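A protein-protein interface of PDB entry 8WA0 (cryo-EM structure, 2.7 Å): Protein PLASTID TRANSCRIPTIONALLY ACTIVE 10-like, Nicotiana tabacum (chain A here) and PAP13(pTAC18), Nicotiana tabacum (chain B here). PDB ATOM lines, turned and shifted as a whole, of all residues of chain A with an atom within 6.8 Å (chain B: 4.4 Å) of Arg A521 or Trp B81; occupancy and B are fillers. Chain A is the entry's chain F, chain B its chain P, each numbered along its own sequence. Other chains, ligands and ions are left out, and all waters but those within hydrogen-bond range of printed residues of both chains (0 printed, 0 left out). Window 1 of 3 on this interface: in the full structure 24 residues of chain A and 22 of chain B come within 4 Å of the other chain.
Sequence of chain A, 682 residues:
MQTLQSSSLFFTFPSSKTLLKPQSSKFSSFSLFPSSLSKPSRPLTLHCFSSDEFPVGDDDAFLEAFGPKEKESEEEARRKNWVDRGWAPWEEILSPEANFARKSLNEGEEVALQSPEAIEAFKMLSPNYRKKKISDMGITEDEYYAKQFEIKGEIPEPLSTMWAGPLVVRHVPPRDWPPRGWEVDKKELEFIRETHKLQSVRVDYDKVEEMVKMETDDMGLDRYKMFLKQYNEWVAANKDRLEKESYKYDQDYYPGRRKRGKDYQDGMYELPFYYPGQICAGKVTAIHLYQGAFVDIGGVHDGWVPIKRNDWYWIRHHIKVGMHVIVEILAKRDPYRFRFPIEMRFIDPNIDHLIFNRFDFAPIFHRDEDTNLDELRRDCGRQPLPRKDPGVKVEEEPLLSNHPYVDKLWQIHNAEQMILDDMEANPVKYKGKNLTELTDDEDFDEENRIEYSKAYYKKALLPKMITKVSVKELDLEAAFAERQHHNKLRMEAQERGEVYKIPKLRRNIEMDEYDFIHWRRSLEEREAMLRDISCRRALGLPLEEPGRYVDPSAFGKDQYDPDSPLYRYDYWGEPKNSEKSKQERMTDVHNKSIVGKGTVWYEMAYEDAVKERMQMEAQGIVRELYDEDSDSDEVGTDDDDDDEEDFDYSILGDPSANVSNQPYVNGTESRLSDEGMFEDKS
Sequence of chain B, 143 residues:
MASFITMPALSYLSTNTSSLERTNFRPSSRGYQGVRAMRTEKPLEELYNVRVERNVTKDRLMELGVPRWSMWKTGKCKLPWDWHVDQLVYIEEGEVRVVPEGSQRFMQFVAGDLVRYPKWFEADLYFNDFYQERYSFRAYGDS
Of the 12 printed residues of chain A, 5 touch a printed residue of chain B. Hydrophobic or aromatic side chains of chain B within 4 Å of the printed part of chain A: Trp B81 and Tyr B135. Among the printed residues, 5 pairs touch across the chains.
Among the printed residues, merely in contact across the chains: Arg A521 with Trp B81 (3.2 Å), Ile A517 with Tyr B135 (3.6 Å) and Arg A520 with Tyr B135 (3.8 Å).
The side-chain carboxylate (OE1) of Glu A525 sits close to the indole nitrogen (NE1) of Trp B81 (3.5 Å). The backbone carbonyl oxygen (O) of Tyr B135 sits close to the side-chain carboxylate (OE2) of Glu A524.
Of the printed residues of chain B, Ile A517 touches Tyr B135 (3.6 Å). Of the printed residues of chain B, Arg A520 touches Tyr B135. Arg A521 touches just one residue of chain B: Trp B81 (3.2 Å). Ser A522 touches none of the printed residues of chain B. Of the printed residues of chain B, Glu A524 touches Tyr B135 (2.8 Å). Of the printed residues of chain B, Glu A525 touches Trp B81 (3.2 Å). Trp B81 touches just these residues of chain A: Arg A521 (3.2 Å) and Glu A525 (3.2 Å). Of the printed residues of chain A, Tyr B135 touches Ile A517, Arg A520 and Glu A524.
The backbone carbonyl oxygen of Ala B123 is in hydrogen-bond range of the backbone NH of Trp B81 (3.4 Å).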
ATOM      1  N   LEU A 400     -23.261  -1.850 -13.037  1.00  0.00           N
ATOM      2  CA  LEU A 400     -23.114  -1.570 -11.624  1.00  0.00           C
ATOM      3  C   LEU A 400     -21.681  -1.169 -11.367  1.00  0.00           C
ATOM      4  O   LEU A 400     -20.760  -1.926 -11.665  1.00  0.00           O
ATOM      5  CB  LEU A 400     -23.477  -2.808 -10.812  1.00  0.00           C
ATOM      6  CG  LEU A 400     -23.774  -2.645  -9.318  1.00  0.00           C
ATOM      7  CD1 LEU A 400     -24.873  -3.600  -8.879  1.00  0.00           C
ATOM      8  CD2 LEU A 400     -22.528  -2.815  -8.459  1.00  0.00           C
ATOM      9  N   PHE A 516     -12.276   0.464  -9.189  1.00  0.00           N
ATOM     10  CA  PHE A 516     -12.061   0.231 -10.586  1.00  0.00           C
ATOM     11  C   PHE A 516     -12.261  -1.188 -11.018  1.00  0.00           C
ATOM     12  O   PHE A 516     -12.799  -1.438 -12.097  1.00  0.00           O
ATOM     13  CB  PHE A 516     -10.685   0.724 -11.029  1.00  0.00           C
ATOM     14  CG  PHE A 516     -10.510   0.736 -12.520  1.00  0.00           C
ATOM     15  CD1 PHE A 516     -11.294   1.558 -13.312  1.00  0.00           C
ATOM     16  CD2 PHE A 516      -9.581  -0.088 -13.132  1.00  0.00           C
ATOM     17  CE1 PHE A 516     -11.153   1.566 -14.684  1.00  0.00           C
ATOM     18  CE2 PHE A 516      -9.432  -0.082 -14.506  1.00  0.00           C
ATOM     19  CZ  PHE A 516     -10.220   0.747 -15.282  1.00  0.00           C
ATOM     20  N   ILE A 517     -11.868  -2.138 -10.197  1.00  0.00           N
ATOM     21  CA  ILE A 517     -11.948  -3.504 -10.671  1.00  0.00           C
ATOM     22  C   ILE A 517     -13.374  -3.853 -11.024  1.00  0.00           C
ATOM     23  O   ILE A 517     -13.618  -4.592 -11.969  1.00  0.00           O
ATOM     24  CB  ILE A 517     -11.321  -4.479  -9.685  1.00  0.00           C
ATOM     25  CG1 ILE A 517     -11.962  -4.372  -8.311  1.00  0.00           C
ATOM     26  CG2 ILE A 517      -9.837  -4.193  -9.549  1.00  0.00           C
ATOM     27  CD1 ILE A 517     -10.952  -4.487  -7.192  1.00  0.00           C
ATOM     28  N   HIS A 518     -14.326  -3.316 -10.283  1.00  0.00           N
ATOM     29  CA  HIS A 518     -15.713  -3.617 -10.512  1.00  0.00           C
ATOM     30  C   HIS A 518     -16.181  -3.210 -11.871  1.00  0.00           C
ATOM     31  O   HIS A 518     -17.028  -3.889 -12.426  1.00  0.00           O
ATOM     32  CB  HIS A 518     -16.571  -2.960  -9.454  1.00  0.00           C
ATOM     33  CG  HIS A 518     -17.607  -3.866  -8.869  1.00  0.00           C
ATOM     34  ND1 HIS A 518     -18.684  -4.330  -9.593  1.00  0.00           N
ATOM     35  CD2 HIS A 518     -17.738  -4.383  -7.625  1.00  0.00           C
ATOM     36  CE1 HIS A 518     -19.429  -5.103  -8.821  1.00  0.00           C
ATOM     37  NE2 HIS A 518     -18.877  -5.150  -7.622  1.00  0.00           N
ATOM     38  N   TRP A 519     -15.713  -2.103 -12.420  1.00  0.00           N
ATOM     39  CA  TRP A 519     -16.263  -1.731 -13.721  1.00  0.00           C
ATOM     40  C   TRP A 519     -15.938  -2.821 -14.694  1.00  0.00           C
ATOM     41  O   TRP A 519     -16.764  -3.202 -15.516  1.00  0.00           O
ATOM     42  CB  TRP A 519     -15.719  -0.428 -14.259  1.00  0.00           C
ATOM     43  CG  TRP A 519     -16.684   0.237 -15.186  1.00  0.00           C
ATOM     44  CD1 TRP A 519     -17.682   1.100 -14.844  1.00  0.00           C
ATOM     45  CD2 TRP A 519     -16.759   0.083 -16.606  1.00  0.00           C
ATOM     46  NE1 TRP A 519     -18.370   1.498 -15.962  1.00  0.00           N
ATOM     47  CE2 TRP A 519     -17.822   0.888 -17.057  1.00  0.00           C
ATOM     48  CE3 TRP A 519     -16.029  -0.652 -17.541  1.00  0.00           C
ATOM     49  CZ2 TRP A 519     -18.173   0.975 -18.396  1.00  0.00           C
ATOM     50  CZ3 TRP A 519     -16.381  -0.564 -18.870  1.00  0.00           C
ATOM     51  CH2 TRP A 519     -17.444   0.243 -19.286  1.00  0.00           C
ATOM     52  N   ARG A 520     -14.740  -3.350 -14.591  1.00  0.00           N
ATOM     53  CA  ARG A 520     -14.344  -4.439 -15.447  1.00  0.00           C
ATOM     54  C   ARG A 520     -15.215  -5.684 -15.222  1.00  0.00           C
ATOM     55  O   ARG A 520     -15.506  -6.425 -16.157  1.00  0.00           O
ATOM     56  CB  ARG A 520     -12.874  -4.734 -15.195  1.00  0.00           C
ATOM     57  CG  ARG A 520     -12.187  -5.546 -16.274  1.00  0.00           C
ATOM     58  CD  ARG A 520     -10.684  -5.512 -16.057  1.00  0.00           C
ATOM     59  NE  ARG A 520     -10.355  -5.592 -14.637  1.00  0.00           N
ATOM     60  CZ  ARG A 520      -9.118  -5.574 -14.153  1.00  0.00           C
ATOM     61  NH1 ARG A 520      -8.915  -5.649 -12.846  1.00  0.00           N
ATOM     62  NH2 ARG A 520      -8.084  -5.481 -14.977  1.00  0.00           N
ATOM     63  N   ARG A 521     -15.609  -5.939 -13.982  1.00  0.00           N
ATOM     64  CA  ARG A 521     -16.412  -7.097 -13.716  1.00  0.00           C
ATOM     65  C   ARG A 521     -17.692  -7.026 -14.467  1.00  0.00           C
ATOM     66  O   ARG A 521     -18.075  -7.992 -15.124  1.00  0.00           O
ATOM     67  CB  ARG A 521     -16.752  -7.144 -12.248  1.00  0.00           C
ATOM     68  CG  ARG A 521     -17.497  -8.392 -11.812  1.00  0.00           C
ATOM     69  CD  ARG A 521     -17.103  -8.814 -10.405  1.00  0.00           C
ATOM     70  NE  ARG A 521     -17.708 -10.089 -10.028  1.00  0.00           N
ATOM     71  CZ  ARG A 521     -18.840 -10.203  -9.342  1.00  0.00           C
ATOM     72  NH1 ARG A 521     -19.320 -11.403  -9.045  1.00  0.00           N
ATOM     73  NH2 ARG A 521     -19.491  -9.119  -8.944  1.00  0.00           N
ATOM     74  N   SER A 522     -18.356  -5.890 -14.432  1.00  0.00           N
ATOM     75  CA  SER A 522     -19.636  -5.830 -15.080  1.00  0.00           C
ATOM     76  C   SER A 522     -19.409  -6.026 -16.504  1.00  0.00           C
ATOM     77  O   SER A 522     -20.150  -6.722 -17.169  1.00  0.00           O
ATOM     78  CB  SER A 522     -20.262  -4.470 -14.937  1.00  0.00           C
ATOM     79  OG  SER A 522     -21.516  -4.433 -15.584  1.00  0.00           O
ATOM     80  N   LEU A 523     -18.375  -5.405 -17.000  1.00  0.00           N
ATOM     81  CA  LEU A 523     -18.148  -5.436 -18.406  1.00  0.00           C
ATOM     82  C   LEU A 523     -17.880  -6.800 -18.875  1.00  0.00           C
ATOM     83  O   LEU A 523     -18.405  -7.232 -19.891  1.00  0.00           O
ATOM     84  CB  LEU A 523     -16.955  -4.545 -18.751  1.00  0.00           C
ATOM     85  CG  LEU A 523     -16.508  -4.494 -20.214  1.00  0.00           C
ATOM     86  CD1 LEU A 523     -17.546  -3.789 -21.074  1.00  0.00           C
ATOM     87  CD2 LEU A 523     -15.155  -3.811 -20.334  1.00  0.00           C
ATOM     88  N   GLU A 524     -17.078  -7.514 -18.129  1.00  0.00           N
ATOM     89  CA  GLU A 524     -16.714  -8.805 -18.647  1.00  0.00           C
ATOM     90  C   GLU A 524     -17.976  -9.623 -18.769  1.00  0.00           C
ATOM     91  O   GLU A 524     -18.240 -10.254 -19.791  1.00  0.00           O
ATOM     92  CB  GLU A 524     -15.711  -9.481 -17.715  1.00  0.00           C
ATOM     93  CG  GLU A 524     -15.015 -10.684 -18.329  1.00  0.00           C
ATOM     94  CD  GLU A 524     -13.919 -11.235 -17.441  1.00  0.00           C
ATOM     95  OE1 GLU A 524     -13.919 -10.924 -16.233  1.00  0.00           O
ATOM     96  OE2 GLU A 524     -13.055 -11.979 -17.952  1.00  0.00           O
ATOM     97  N   GLU A 525     -18.790  -9.570 -17.739  1.00  0.00           N
ATOM     98  CA  GLU A 525     -19.987 -10.334 -17.755  1.00  0.00           C
ATOM     99  C   GLU A 525     -20.940  -9.915 -18.804  1.00  0.00           C
ATOM    100  O   GLU A 525     -21.466 -10.745 -19.511  1.00  0.00           O
ATOM    101  CB  GLU A 525     -20.650 -10.155 -16.396  1.00  0.00           C
ATOM    102  CG  GLU A 525     -22.080 -10.651 -16.293  1.00  0.00           C
ATOM    103  CD  GLU A 525     -22.629 -10.552 -14.884  1.00  0.00           C
ATOM    104  OE1 GLU A 525     -21.929  -9.994 -14.013  1.00  0.00           O
ATOM    105  OE2 GLU A 525     -23.758 -11.031 -14.648  1.00  0.00           O
ATOM    106  N   ARG A 526     -21.165  -8.638 -18.950  1.00  0.00           N
ATOM    107  CA  ARG A 526     -22.182  -8.221 -19.858  1.00  0.00           C
ATOM    108  C   ARG A 526     -21.834  -8.615 -21.244  1.00  0.00           C
ATOM    109  O   ARG A 526     -22.679  -8.961 -22.044  1.00  0.00           O
ATOM    110  CB  ARG A 526     -22.446  -6.757 -19.715  1.00  0.00           C
ATOM    111  N   LEU B  79     -20.761  -9.787  -0.482  1.00  0.00           N
ATOM    112  CA  LEU B  79     -21.328  -9.393  -1.751  1.00  0.00           C
ATOM    113  C   LEU B  79     -22.467 -10.266  -2.170  1.00  0.00           C
ATOM    114  O   LEU B  79     -22.352 -11.476  -2.208  1.00  0.00           O
ATOM    115  CB  LEU B  79     -20.258  -9.523  -2.827  1.00  0.00           C
ATOM    116  N   PRO B  80     -23.571  -9.660  -2.531  1.00  0.00           N
ATOM    117  CA  PRO B  80     -24.619 -10.490  -3.089  1.00  0.00           C
ATOM    118  C   PRO B  80     -24.536 -10.465  -4.591  1.00  0.00           C
ATOM    119  O   PRO B  80     -24.747  -9.410  -5.174  1.00  0.00           O
ATOM    120  CB  PRO B  80     -25.886  -9.741  -2.695  1.00  0.00           C
ATOM    121  CG  PRO B  80     -25.491  -8.790  -1.617  1.00  0.00           C
ATOM    122  CD  PRO B  80     -24.094  -8.410  -1.966  1.00  0.00           C
ATOM    123  N   TRP B  81     -24.284 -11.608  -5.217  1.00  0.00           N
ATOM    124  CA  TRP B  81     -24.237 -11.664  -6.664  1.00  0.00           C
ATOM    125  C   TRP B  81     -25.053 -12.742  -7.312  1.00  0.00           C
ATOM    126  O   TRP B  81     -25.156 -13.833  -6.789  1.00  0.00           O
ATOM    127  CB  TRP B  81     -22.810 -11.771  -7.166  1.00  0.00           C
ATOM    128  CG  TRP B  81     -22.651 -11.269  -8.551  1.00  0.00           C
ATOM    129  CD1 TRP B  81     -22.510 -12.010  -9.683  1.00  0.00           C
ATOM    130  CD2 TRP B  81     -22.637  -9.904  -8.959  1.00  0.00           C
ATOM    131  NE1 TRP B  81     -22.398 -11.187 -10.773  1.00  0.00           N
ATOM    132  CE2 TRP B  81     -22.473  -9.886 -10.353  1.00  0.00           C
ATOM    133  CE3 TRP B  81     -22.736  -8.688  -8.276  1.00  0.00           C
ATOM    134  CZ2 TRP B  81     -22.408  -8.706 -11.076  1.00  0.00           C
ATOM    135  CZ3 TRP B  81     -22.672  -7.520  -8.995  1.00  0.00           C
ATOM    136  CH2 TRP B  81     -22.503  -7.535 -10.379  1.00  0.00           C
ATOM    137  N   ASP B  82     -25.645 -12.432  -8.455  1.00  0.00           N
ATOM    138  CA  ASP B  82     -26.391 -13.397  -9.203  1.00  0.00           C
ATOM    139  C   ASP B  82     -25.660 -13.504 -10.501  1.00  0.00           C
ATOM    140  O   ASP B  82     -25.537 -12.519 -11.221  1.00  0.00           O
ATOM    141  CB  ASP B  82     -27.770 -12.829  -9.423  1.00  0.00           C
ATOM    142  CG  ASP B  82     -28.679 -13.753 -10.226  1.00  0.00           C
ATOM    143  OD1 ASP B  82     -28.283 -14.894 -10.545  1.00  0.00           O
ATOM    144  OD2 ASP B  82     -29.810 -13.329 -10.538  1.00  0.00           O
ATOM    145  N   TRP B  83     -25.187 -14.684 -10.845  1.00  0.00           N
ATOM    146  CA  TRP B  83     -24.398 -14.824 -12.027  1.00  0.00           C
ATOM    147  C   TRP B  83     -25.293 -15.117 -13.190  1.00  0.00           C
ATOM    148  O   TRP B  83     -25.962 -16.134 -13.197  1.00  0.00           O
ATOM    149  CB  TRP B  83     -23.441 -15.966 -11.826  1.00  0.00           C
ATOM    150  CG  TRP B  83     -22.380 -15.791 -10.821  1.00  0.00           C
ATOM    151  CD1 TRP B  83     -21.085 -15.478 -11.066  1.00  0.00           C
ATOM    152  CD2 TRP B  83     -22.489 -15.972  -9.408  1.00  0.00           C
ATOM    153  NE1 TRP B  83     -20.379 -15.431  -9.894  1.00  0.00           N
ATOM    154  CE2 TRP B  83     -21.222 -15.735  -8.861  1.00  0.00           C
ATOM    155  CE3 TRP B  83     -23.536 -16.308  -8.553  1.00  0.00           C
ATOM    156  CZ2 TRP B  83     -20.974 -15.813  -7.499  1.00  0.00           C
ATOM    157  CZ3 TRP B  83     -23.290 -16.387  -7.202  1.00  0.00           C
ATOM    158  CH2 TRP B  83     -22.020 -16.140  -6.686  1.00  0.00           C
ATOM    159  N   GLN B  87     -18.745 -18.247 -14.535  1.00  0.00           N
ATOM    160  CA  GLN B  87     -17.484 -17.580 -14.232  1.00  0.00           C
ATOM    161  C   GLN B  87     -16.470 -18.579 -13.880  1.00  0.00           C
ATOM    162  O   GLN B  87     -16.738 -19.445 -13.063  1.00  0.00           O
ATOM    163  CB  GLN B  87     -17.637 -16.712 -13.005  1.00  0.00           C
ATOM    164  CG  GLN B  87     -16.597 -15.619 -12.880  1.00  0.00           C
ATOM    165  CD  GLN B  87     -16.810 -14.766 -11.648  1.00  0.00           C
ATOM    166  OE1 GLN B  87     -17.530 -15.154 -10.729  1.00  0.00           O
ATOM    167  NE2 GLN B  87     -16.180 -13.599 -11.619  1.00  0.00           N
ATOM    168  N   PHE B 121     -27.136 -19.046 -11.020  1.00  0.00           N
ATOM    169  CA  PHE B 121     -26.826 -19.210  -9.600  1.00  0.00           C
ATOM    170  C   PHE B 121     -26.978 -17.922  -8.837  1.00  0.00           C
ATOM    171  O   PHE B 121     -26.588 -16.875  -9.319  1.00  0.00           O
ATOM    172  CB  PHE B 121     -25.408 -19.704  -9.410  1.00  0.00           C
ATOM    173  CG  PHE B 121     -25.083 -20.125  -8.009  1.00  0.00           C
ATOM    174  CD1 PHE B 121     -25.973 -20.877  -7.269  1.00  0.00           C
ATOM    175  CD2 PHE B 121     -23.865 -19.800  -7.446  1.00  0.00           C
ATOM    176  CE1 PHE B 121     -25.665 -21.269  -5.982  1.00  0.00           C
ATOM    177  CE2 PHE B 121     -23.547 -20.193  -6.164  1.00  0.00           C
ATOM    178  CZ  PHE B 121     -24.449 -20.932  -5.431  1.00  0.00           C
ATOM    179  N   GLU B 122     -27.525 -17.996  -7.637  1.00  0.00           N
ATOM    180  CA  GLU B 122     -27.682 -16.819  -6.804  1.00  0.00           C
ATOM    181  C   GLU B 122     -27.250 -17.186  -5.402  1.00  0.00           C
ATOM    182  O   GLU B 122     -27.803 -18.110  -4.812  1.00  0.00           O
ATOM    183  CB  GLU B 122     -29.142 -16.392  -6.738  1.00  0.00           C
ATOM    184  CG  GLU B 122     -29.877 -16.316  -8.059  1.00  0.00           C
ATOM    185  CD  GLU B 122     -31.272 -15.755  -7.902  1.00  0.00           C
ATOM    186  OE1 GLU B 122     -31.652 -15.429  -6.758  1.00  0.00           O
ATOM    187  OE2 GLU B 122     -31.988 -15.640  -8.918  1.00  0.00           O
ATOM    188  N   ALA B 123     -26.290 -16.463  -4.848  1.00  0.00           N
ATOM    189  CA  ALA B 123     -25.780 -16.790  -3.527  1.00  0.00           C
ATOM    190  C   ALA B 123     -25.119 -15.578  -2.946  1.00  0.00           C
ATOM    191  O   ALA B 123     -24.921 -14.590  -3.648  1.00  0.00           O
ATOM    192  CB  ALA B 123     -24.776 -17.889  -3.611  1.00  0.00           C
ATOM    193  N   LEU B 125     -21.670 -13.944  -1.176  1.00  0.00           N
ATOM    194  CA  LEU B 125     -20.256 -14.236  -1.024  1.00  0.00           C
ATOM    195  C   LEU B 125     -19.666 -13.449   0.099  1.00  0.00           C
ATOM    196  O   LEU B 125     -19.649 -12.234   0.046  1.00  0.00           O
ATOM    197  CB  LEU B 125     -19.576 -13.836  -2.303  1.00  0.00           C
ATOM    198  CG  LEU B 125     -20.135 -14.405  -3.597  1.00  0.00           C
ATOM    199  CD1 LEU B 125     -19.734 -13.526  -4.768  1.00  0.00           C
ATOM    200  CD2 LEU B 125     -19.659 -15.833  -3.794  1.00  0.00           C
ATOM    201  N   TYR B 135     -10.543 -13.858 -13.094  1.00  0.00           N
ATOM    202  CA  TYR B 135     -11.847 -14.208 -13.620  1.00  0.00           C
ATOM    203  C   TYR B 135     -12.091 -14.197 -15.094  1.00  0.00           C
ATOM    204  O   TYR B 135     -11.821 -13.200 -15.730  1.00  0.00           O
ATOM    205  CB  TYR B 135     -12.926 -13.364 -12.946  1.00  0.00           C
ATOM    206  CG  TYR B 135     -12.670 -11.896 -12.722  1.00  0.00           C
ATOM    207  CD1 TYR B 135     -11.775 -11.455 -11.766  1.00  0.00           C
ATOM    208  CD2 TYR B 135     -13.405 -10.946 -13.400  1.00  0.00           C
ATOM    209  CE1 TYR B 135     -11.571 -10.111 -11.554  1.00  0.00           C
ATOM    210  CE2 TYR B 135     -13.209  -9.597 -13.197  1.00  0.00           C
ATOM    211  CZ  TYR B 135     -12.291  -9.183 -12.266  1.00  0.00           C
ATOM    212  OH  TYR B 135     -12.092  -7.839 -12.054  1.00  0.00           O
